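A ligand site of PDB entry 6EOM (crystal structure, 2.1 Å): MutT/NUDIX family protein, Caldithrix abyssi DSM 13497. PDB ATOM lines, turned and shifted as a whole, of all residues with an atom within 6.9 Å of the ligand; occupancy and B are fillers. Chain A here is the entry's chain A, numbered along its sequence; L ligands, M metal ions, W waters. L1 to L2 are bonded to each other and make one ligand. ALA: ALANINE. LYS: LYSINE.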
ATOM      1  N   ASP A 310      -9.297   2.077  13.225  1.00  0.00           N
ATOM      2  CA  ASP A 310      -9.229   1.312  11.977  1.00  0.00           C
ATOM      3  C   ASP A 310      -8.388   2.022  10.921  1.00  0.00           C
ATOM      4  O   ASP A 310      -7.564   1.393  10.245  1.00  0.00           O
ATOM      5  CB  ASP A 310     -10.644   1.060  11.452  1.00  0.00           C
ATOM      6  CG  ASP A 310     -10.656   0.273  10.157  1.00  0.00           C
ATOM      7  OD1 ASP A 310      -9.688  -0.467   9.886  1.00  0.00           O
ATOM      8  OD2 ASP A 310     -11.642   0.407   9.394  1.00  0.00           O
ATOM      9  N   THR A 311      -8.558   3.338  10.772  1.00  0.00           N
ATOM     10  CA  THR A 311      -7.915   4.039   9.671  1.00  0.00           C
ATOM     11  C   THR A 311      -6.405   4.152   9.865  1.00  0.00           C
ATOM     12  O   THR A 311      -5.663   4.193   8.882  1.00  0.00           O
ATOM     13  CB  THR A 311      -8.524   5.435   9.501  1.00  0.00           C
ATOM     14  OG1 THR A 311      -7.862   6.114   8.420  1.00  0.00           O
ATOM     15  CG2 THR A 311      -8.389   6.249  10.778  1.00  0.00           C
ATOM     16  N   ALA A 313      -4.345   1.948  11.099  1.00  0.00           N
ATOM     17  CA  ALA A 313      -3.621   0.698  10.880  1.00  0.00           C
ATOM     18  C   ALA A 313      -3.086   0.634   9.452  1.00  0.00           C
ATOM     19  O   ALA A 313      -3.771   1.001   8.491  1.00  0.00           O
ATOM     20  CB  ALA A 313      -4.528  -0.499  11.149  1.00  0.00           C
ATOM     21  N   VAL A 315      -1.734   1.148   5.958  1.00  0.00           N
ATOM     22  CA  VAL A 315      -1.667   2.268   5.022  1.00  0.00           C
ATOM     23  C   VAL A 315      -2.654   3.339   5.459  1.00  0.00           C
ATOM     24  O   VAL A 315      -3.779   3.041   5.894  1.00  0.00           O
ATOM     25  CB  VAL A 315      -1.950   1.781   3.591  1.00  0.00           C
ATOM     26  CG1 VAL A 315      -2.182   2.945   2.654  1.00  0.00           C
ATOM     27  CG2 VAL A 315      -0.814   0.901   3.094  1.00  0.00           C
ATOM     28  N   GLN A 316      -2.252   4.601   5.313  1.00  0.00           N
ATOM     29  CA  GLN A 316      -3.043   5.724   5.793  1.00  0.00           C
ATOM     30  C   GLN A 316      -4.072   6.168   4.757  1.00  0.00           C
ATOM     31  O   GLN A 316      -3.878   6.021   3.549  1.00  0.00           O
ATOM     32  CB  GLN A 316      -2.136   6.896   6.161  1.00  0.00           C
ATOM     33  CG  GLN A 316      -1.123   6.535   7.230  1.00  0.00           C
ATOM     34  CD  GLN A 316      -1.770   5.878   8.422  1.00  0.00           C
ATOM     35  OE1 GLN A 316      -2.669   6.432   9.047  1.00  0.00           O
ATOM     36  NE2 GLN A 316      -1.321   4.671   8.741  1.00  0.00           N
ATOM     37  N   THR A 317      -5.166   6.736   5.263  1.00  0.00           N
ATOM     38  CA  THR A 317      -6.250   7.197   4.426  1.00  0.00           C
ATOM     39  C   THR A 317      -5.928   8.566   3.833  1.00  0.00           C
ATOM     40  O   THR A 317      -5.434   9.452   4.538  1.00  0.00           O
ATOM     41  CB  THR A 317      -7.550   7.257   5.222  1.00  0.00           C
ATOM     42  OG1 THR A 317      -7.850   5.959   5.757  1.00  0.00           O
ATOM     43  CG2 THR A 317      -8.708   7.724   4.351  1.00  0.00           C
ATOM     44  N   LEU A 318      -6.202   8.718   2.542  1.00  0.00           N
ATOM     45  CA  LEU A 318      -6.099  10.022   1.882  1.00  0.00           C
ATOM     46  C   LEU A 318      -7.405  10.797   1.908  1.00  0.00           C
ATOM     47  O   LEU A 318      -7.379  12.029   1.884  1.00  0.00           O
ATOM     48  CB  LEU A 318      -5.654   9.845   0.423  1.00  0.00           C
ATOM     49  CG  LEU A 318      -4.179   9.545   0.171  1.00  0.00           C
ATOM     50  CD1 LEU A 318      -3.927   9.403  -1.323  1.00  0.00           C
ATOM     51  CD2 LEU A 318      -3.306  10.641   0.764  1.00  0.00           C
ATOM     52  N   ALA A 319      -8.534  10.104   1.978  1.00  0.00           N
ATOM     53  CA  ALA A 319      -9.863  10.710   2.004  1.00  0.00           C
ATOM     54  C   ALA A 319     -10.869   9.623   2.342  1.00  0.00           C
ATOM     55  O   ALA A 319     -10.713   8.476   1.924  1.00  0.00           O
ATOM     56  CB  ALA A 319     -10.213  11.352   0.646  1.00  0.00           C
ATOM     57  N   PHE A 320     -11.900   9.984   3.105  1.00  0.00           N
ATOM     58  CA  PHE A 320     -12.924   9.025   3.487  1.00  0.00           C
ATOM     59  C   PHE A 320     -14.303   9.552   3.090  1.00  0.00           C
ATOM     60  O   PHE A 320     -14.490  10.734   2.775  1.00  0.00           O
ATOM     61  CB  PHE A 320     -12.881   8.704   4.990  1.00  0.00           C
ATOM     62  CG  PHE A 320     -12.944   9.896   5.894  1.00  0.00           C
ATOM     63  CD1 PHE A 320     -14.155  10.323   6.426  1.00  0.00           C
ATOM     64  CD2 PHE A 320     -11.796  10.587   6.244  1.00  0.00           C
ATOM     65  CE1 PHE A 320     -14.219  11.410   7.266  1.00  0.00           C
ATOM     66  CE2 PHE A 320     -11.848  11.680   7.090  1.00  0.00           C
ATOM     67  CZ  PHE A 320     -13.064  12.093   7.608  1.00  0.00           C
ATOM     68  N   HIS A 343      -2.090  14.080   2.007  1.00  0.00           N
ATOM     69  CA  HIS A 343      -1.647  14.137   0.618  1.00  0.00           C
ATOM     70  C   HIS A 343      -0.251  14.738   0.507  1.00  0.00           C
ATOM     71  O   HIS A 343       0.580  14.258  -0.265  1.00  0.00           O
ATOM     72  CB  HIS A 343      -2.636  14.943  -0.227  1.00  0.00           C
ATOM     73  CG  HIS A 343      -3.827  14.163  -0.679  1.00  0.00           C
ATOM     74  ND1 HIS A 343      -4.886  13.854   0.155  1.00  0.00           N
ATOM     75  CD2 HIS A 343      -4.149  13.648  -1.896  1.00  0.00           C
ATOM     76  CE1 HIS A 343      -5.796  13.177  -0.525  1.00  0.00           C
ATOM     77  NE2 HIS A 343      -5.372  13.035  -1.770  1.00  0.00           N
ATOM     78  N   LYS A 346       2.279  12.098   1.562  1.00  0.00           N
ATOM     79  CA  LYS A 346       2.430  11.039   0.574  1.00  0.00           C
ATOM     80  C   LYS A 346       3.078  11.553  -0.702  1.00  0.00           C
ATOM     81  O   LYS A 346       3.852  10.832  -1.350  1.00  0.00           O
ATOM     82  CB  LYS A 346       1.063  10.413   0.268  1.00  0.00           C
ATOM     83  CG  LYS A 346       0.456   9.672   1.454  1.00  0.00           C
ATOM     84  CD  LYS A 346      -0.173   8.347   1.033  1.00  0.00           C
ATOM     85  CE  LYS A 346      -1.271   7.933   2.001  1.00  0.00           C
ATOM     86  NZ  LYS A 346      -1.521   6.458   1.949  1.00  0.00           N
ATOM     87  N   LEU A 350       6.477   9.694  -1.247  1.00  0.00           N
ATOM     88  CA  LEU A 350       6.185   8.549  -2.109  1.00  0.00           C
ATOM     89  C   LEU A 350       6.042   8.928  -3.575  1.00  0.00           C
ATOM     90  O   LEU A 350       6.792   8.431  -4.414  1.00  0.00           O
ATOM     91  CB  LEU A 350       4.912   7.857  -1.628  1.00  0.00           C
ATOM     92  CG  LEU A 350       4.969   7.373  -0.173  1.00  0.00           C
ATOM     93  CD1 LEU A 350       3.604   6.979   0.313  1.00  0.00           C
ATOM     94  CD2 LEU A 350       5.949   6.214  -0.053  1.00  0.00           C
ATOM     95  N   PHE A 372      -1.761  15.817  -7.914  1.00  0.00           N
ATOM     96  CA  PHE A 372      -2.067  14.699  -7.026  1.00  0.00           C
ATOM     97  C   PHE A 372      -3.341  14.957  -6.232  1.00  0.00           C
ATOM     98  O   PHE A 372      -4.240  14.110  -6.203  1.00  0.00           O
ATOM     99  CB  PHE A 372      -0.882  14.450  -6.087  1.00  0.00           C
ATOM    100  CG  PHE A 372      -1.090  13.313  -5.125  1.00  0.00           C
ATOM    101  CD1 PHE A 372      -1.642  12.115  -5.544  1.00  0.00           C
ATOM    102  CD2 PHE A 372      -0.705  13.436  -3.796  1.00  0.00           C
ATOM    103  CE1 PHE A 372      -1.826  11.075  -4.655  1.00  0.00           C
ATOM    104  CE2 PHE A 372      -0.889  12.396  -2.908  1.00  0.00           C
ATOM    105  CZ  PHE A 372      -1.448  11.220  -3.334  1.00  0.00           C
ATOM    106  N   THR A 376      -7.579  13.295  -6.752  1.00  0.00           N
ATOM    107  CA  THR A 376      -8.380  12.673  -5.700  1.00  0.00           C
ATOM    108  C   THR A 376      -9.722  13.371  -5.543  1.00  0.00           C
ATOM    109  O   THR A 376     -10.754  12.716  -5.388  1.00  0.00           O
ATOM    110  CB  THR A 376      -7.603  12.684  -4.377  1.00  0.00           C
ATOM    111  OG1 THR A 376      -6.413  11.893  -4.509  1.00  0.00           O
ATOM    112  CG2 THR A 376      -8.459  12.118  -3.251  1.00  0.00           C
ATOM    113  N   HIS A 379     -11.580  12.328  -8.614  1.00  0.00           N
ATOM    114  CA  HIS A 379     -11.847  10.897  -8.510  1.00  0.00           C
ATOM    115  C   HIS A 379     -13.068  10.632  -7.637  1.00  0.00           C
ATOM    116  O   HIS A 379     -13.936   9.822  -7.985  1.00  0.00           O
ATOM    117  CB  HIS A 379     -10.617  10.173  -7.951  1.00  0.00           C
ATOM    118  CG  HIS A 379     -10.832   8.724  -7.652  1.00  0.00           C
ATOM    119  ND1 HIS A 379     -10.182   7.715  -8.336  1.00  0.00           N
ATOM    120  CD2 HIS A 379     -11.585   8.108  -6.714  1.00  0.00           C
ATOM    121  CE1 HIS A 379     -10.552   6.543  -7.851  1.00  0.00           C
ATOM    122  NE2 HIS A 379     -11.404   6.751  -6.864  1.00  0.00           N
ATOM    123  N   GLU A 380     -13.149  11.318  -6.495  1.00  0.00           N
ATOM    124  CA  GLU A 380     -14.304  11.161  -5.609  1.00  0.00           C
ATOM    125  C   GLU A 380     -15.567  11.716  -6.259  1.00  0.00           C
ATOM    126  O   GLU A 380     -16.631  11.102  -6.160  1.00  0.00           O
ATOM    127  CB  GLU A 380     -14.036  11.856  -4.277  1.00  0.00           C
ATOM    128  CG  GLU A 380     -13.031  11.137  -3.397  1.00  0.00           C
ATOM    129  CD  GLU A 380     -13.430   9.701  -3.111  1.00  0.00           C
ATOM    130  OE1 GLU A 380     -12.721   8.783  -3.573  1.00  0.00           O
ATOM    131  OE2 GLU A 380     -14.454   9.496  -2.438  1.00  0.00           O
ATOM    132  N   GLU A 412     -13.623   1.746  -9.973  1.00  0.00           N
ATOM    133  CA  GLU A 412     -12.421   2.526  -9.679  1.00  0.00           C
ATOM    134  C   GLU A 412     -11.695   2.931 -10.957  1.00  0.00           C
ATOM    135  O   GLU A 412     -11.073   4.002 -11.003  1.00  0.00           O
ATOM    136  CB  GLU A 412     -11.490   1.741  -8.750  1.00  0.00           C
ATOM    137  CG  GLU A 412     -11.954   1.712  -7.310  1.00  0.00           C
ATOM    138  CD  GLU A 412     -12.087   3.095  -6.703  1.00  0.00           C
ATOM    139  OE1 GLU A 412     -11.271   3.975  -7.046  1.00  0.00           O
ATOM    140  OE2 GLU A 412     -13.010   3.317  -5.901  1.00  0.00           O
ATOM    141  N   ARG A 450       2.400   4.288  -7.707  1.00  0.00           N
ATOM    142  CA  ARG A 450       2.227   4.303  -6.257  1.00  0.00           C
ATOM    143  C   ARG A 450       1.061   3.413  -5.855  1.00  0.00           C
ATOM    144  O   ARG A 450       1.160   2.623  -4.913  1.00  0.00           O
ATOM    145  CB  ARG A 450       2.006   5.730  -5.757  1.00  0.00           C
ATOM    146  CG  ARG A 450       1.854   5.841  -4.238  1.00  0.00           C
ATOM    147  CD  ARG A 450       1.406   7.232  -3.806  1.00  0.00           C
ATOM    148  NE  ARG A 450       0.026   7.497  -4.178  1.00  0.00           N
ATOM    149  CZ  ARG A 450      -1.024   7.173  -3.422  1.00  0.00           C
ATOM    150  NH1 ARG A 450      -0.855   6.565  -2.258  1.00  0.00           N
ATOM    151  NH2 ARG A 450      -2.254   7.458  -3.843  1.00  0.00           N
ATOM    152  N   THR A 451      -0.056   3.522  -6.585  1.00  0.00           N
ATOM    153  CA  THR A 451      -1.233   2.724  -6.288  1.00  0.00           C
ATOM    154  C   THR A 451      -0.976   1.238  -6.511  1.00  0.00           C
ATOM    155  O   THR A 451      -1.385   0.399  -5.687  1.00  0.00           O
ATOM    156  CB  THR A 451      -2.409   3.195  -7.143  1.00  0.00           C
ATOM    157  OG1 THR A 451      -2.723   4.553  -6.833  1.00  0.00           O
ATOM    158  CG2 THR A 451      -3.634   2.319  -6.913  1.00  0.00           C
ATOM    159  N   PHE A 454       0.542  -1.253  -3.952  1.00  0.00           N
ATOM    160  CA  PHE A 454      -0.314  -1.819  -2.918  1.00  0.00           C
ATOM    161  C   PHE A 454      -0.843  -3.195  -3.292  1.00  0.00           C
ATOM    162  O   PHE A 454      -1.254  -3.956  -2.401  1.00  0.00           O
ATOM    163  CB  PHE A 454      -1.488  -0.881  -2.634  1.00  0.00           C
ATOM    164  CG  PHE A 454      -1.089   0.413  -1.974  1.00  0.00           C
ATOM    165  CD1 PHE A 454      -0.165   0.416  -0.948  1.00  0.00           C
ATOM    166  CD2 PHE A 454      -1.649   1.612  -2.379  1.00  0.00           C
ATOM    167  CE1 PHE A 454       0.204   1.603  -0.341  1.00  0.00           C
ATOM    168  CE2 PHE A 454      -1.281   2.798  -1.772  1.00  0.00           C
ATOM    169  CZ  PHE A 454      -0.359   2.794  -0.753  1.00  0.00           C
ATOM    170  N   HIS A 460      -8.756  -0.919  -6.804  1.00  0.00           N
ATOM    171  CA  HIS A 460      -8.099   0.308  -7.244  1.00  0.00           C
ATOM    172  C   HIS A 460      -6.853   0.003  -8.053  1.00  0.00           C
ATOM    173  O   HIS A 460      -6.618   0.637  -9.091  1.00  0.00           O
ATOM    174  CB  HIS A 460      -7.772   1.171  -6.031  1.00  0.00           C
ATOM    175  CG  HIS A 460      -7.396   2.576  -6.383  1.00  0.00           C
ATOM    176  ND1 HIS A 460      -6.690   3.406  -5.530  1.00  0.00           N
ATOM    177  CD2 HIS A 460      -7.633   3.318  -7.497  1.00  0.00           C
ATOM    178  CE1 HIS A 460      -6.512   4.579  -6.105  1.00  0.00           C
ATOM    179  NE2 HIS A 460      -7.072   4.553  -7.297  1.00  0.00           N
ATOM    180  N   ASP A 543       4.223   3.091   2.218  1.00  0.00           N
ATOM    181  CA  ASP A 543       3.360   4.189   2.638  1.00  0.00           C
ATOM    182  C   ASP A 543       4.062   5.036   3.690  1.00  0.00           C
ATOM    183  O   ASP A 543       5.277   5.246   3.600  1.00  0.00           O
ATOM    184  CB  ASP A 543       2.023   3.652   3.173  1.00  0.00           C
ATOM    185  CG  ASP A 543       0.915   4.704   3.119  1.00  0.00           C
ATOM    186  OD1 ASP A 543       0.674   5.248   2.019  1.00  0.00           O
ATOM    187  OD2 ASP A 543       0.303   4.981   4.163  1.00  0.00           O
HETATM  188  N   ALA L   1      -9.018   4.364  -0.321  1.00  0.00           N
HETATM  189  CA  ALA L   1      -8.484   5.577  -0.930  1.00  0.00           C
HETATM  190  C   ALA L   1      -7.328   6.150  -0.116  1.00  0.00           C
HETATM  191  O   ALA L   1      -7.546   6.846   0.878  1.00  0.00           O
HETATM  192  CB  ALA L   1      -9.584   6.619  -1.085  1.00  0.00           C
HETATM  193  N   LYS L   2      -6.310   5.187  -0.407  1.00  0.00           N
HETATM  194  CA  LYS L   2      -4.933   5.000   0.031  1.00  0.00           C
HETATM  195  C   LYS L   2      -3.976   5.804  -0.839  1.00  0.00           C
HETATM  196  O   LYS L   2      -2.875   6.157  -0.424  1.00  0.00           O
HETATM  197  CB  LYS L   2      -4.553   3.514  -0.007  1.00  0.00           C
HETATM  198  CG  LYS L   2      -5.545   2.600   0.690  1.00  0.00           C
HETATM  199  CD  LYS L   2      -5.805   3.052   2.120  1.00  0.00           C
HETATM  200  CE  LYS L   2      -6.941   2.271   2.747  1.00  0.00           C
HETATM  201  NZ  LYS L   2      -7.217   2.708   4.138  1.00  0.00           N
HETATM  202  OXT LYS L   2      -4.292   6.124  -1.985  1.00  0.00           O
HETATM  203 ZN    ZN M   1     -12.367   5.224  -5.929  1.00  0.00          ZN
HETATM  204  O   HOH W   1      -5.719   6.944  -3.804  1.00  0.00           O
HETATM  205  O   HOH W   2     -11.725   2.965  -0.203  1.00  0.00           O
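O of LYS L2 lies within salt-bridge range of NZ of Lys 346, 2.7 Å away.
An oxygen (O) of LYS L2 lies within salt-bridge range of the guanidinium group (NH1) of Arg 450.
The backbone NH of Leu 318 is in hydrogen-bond range of an oxygen (O) of ALA L1, at 2.8 Å.
The side-chain amino group (NZ) of Lys 346 lies within hydrogen-bond range of the backbone carbonyl oxygen (O) of Gln 316, 2.9 Å away.
NZ of Lys 346 is in salt-bridge range of OD1 of Asp 543 (2.5 Å).
The side-chain hydroxyl (OG1) of Thr 317 lies within hydrogen-bond range of the side-chain hydroxyl (OG1) of Thr 311, at 2.7 Å.
The side-chain carboxylate of Asp 543 is in hydrogen-bond range of the backbone NH of Gln 316, 2.8 Å away.
Residues that only touch the ligand: Val 315 (3.6 Å), Gln 316 (3.8 Å), Thr 317 (3.7 Å), Ala 319 (3.6 Å) and Phe 454 (3.8 Å).
Of the 22 residues printed, 8 come within 4 Å of the ligand.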
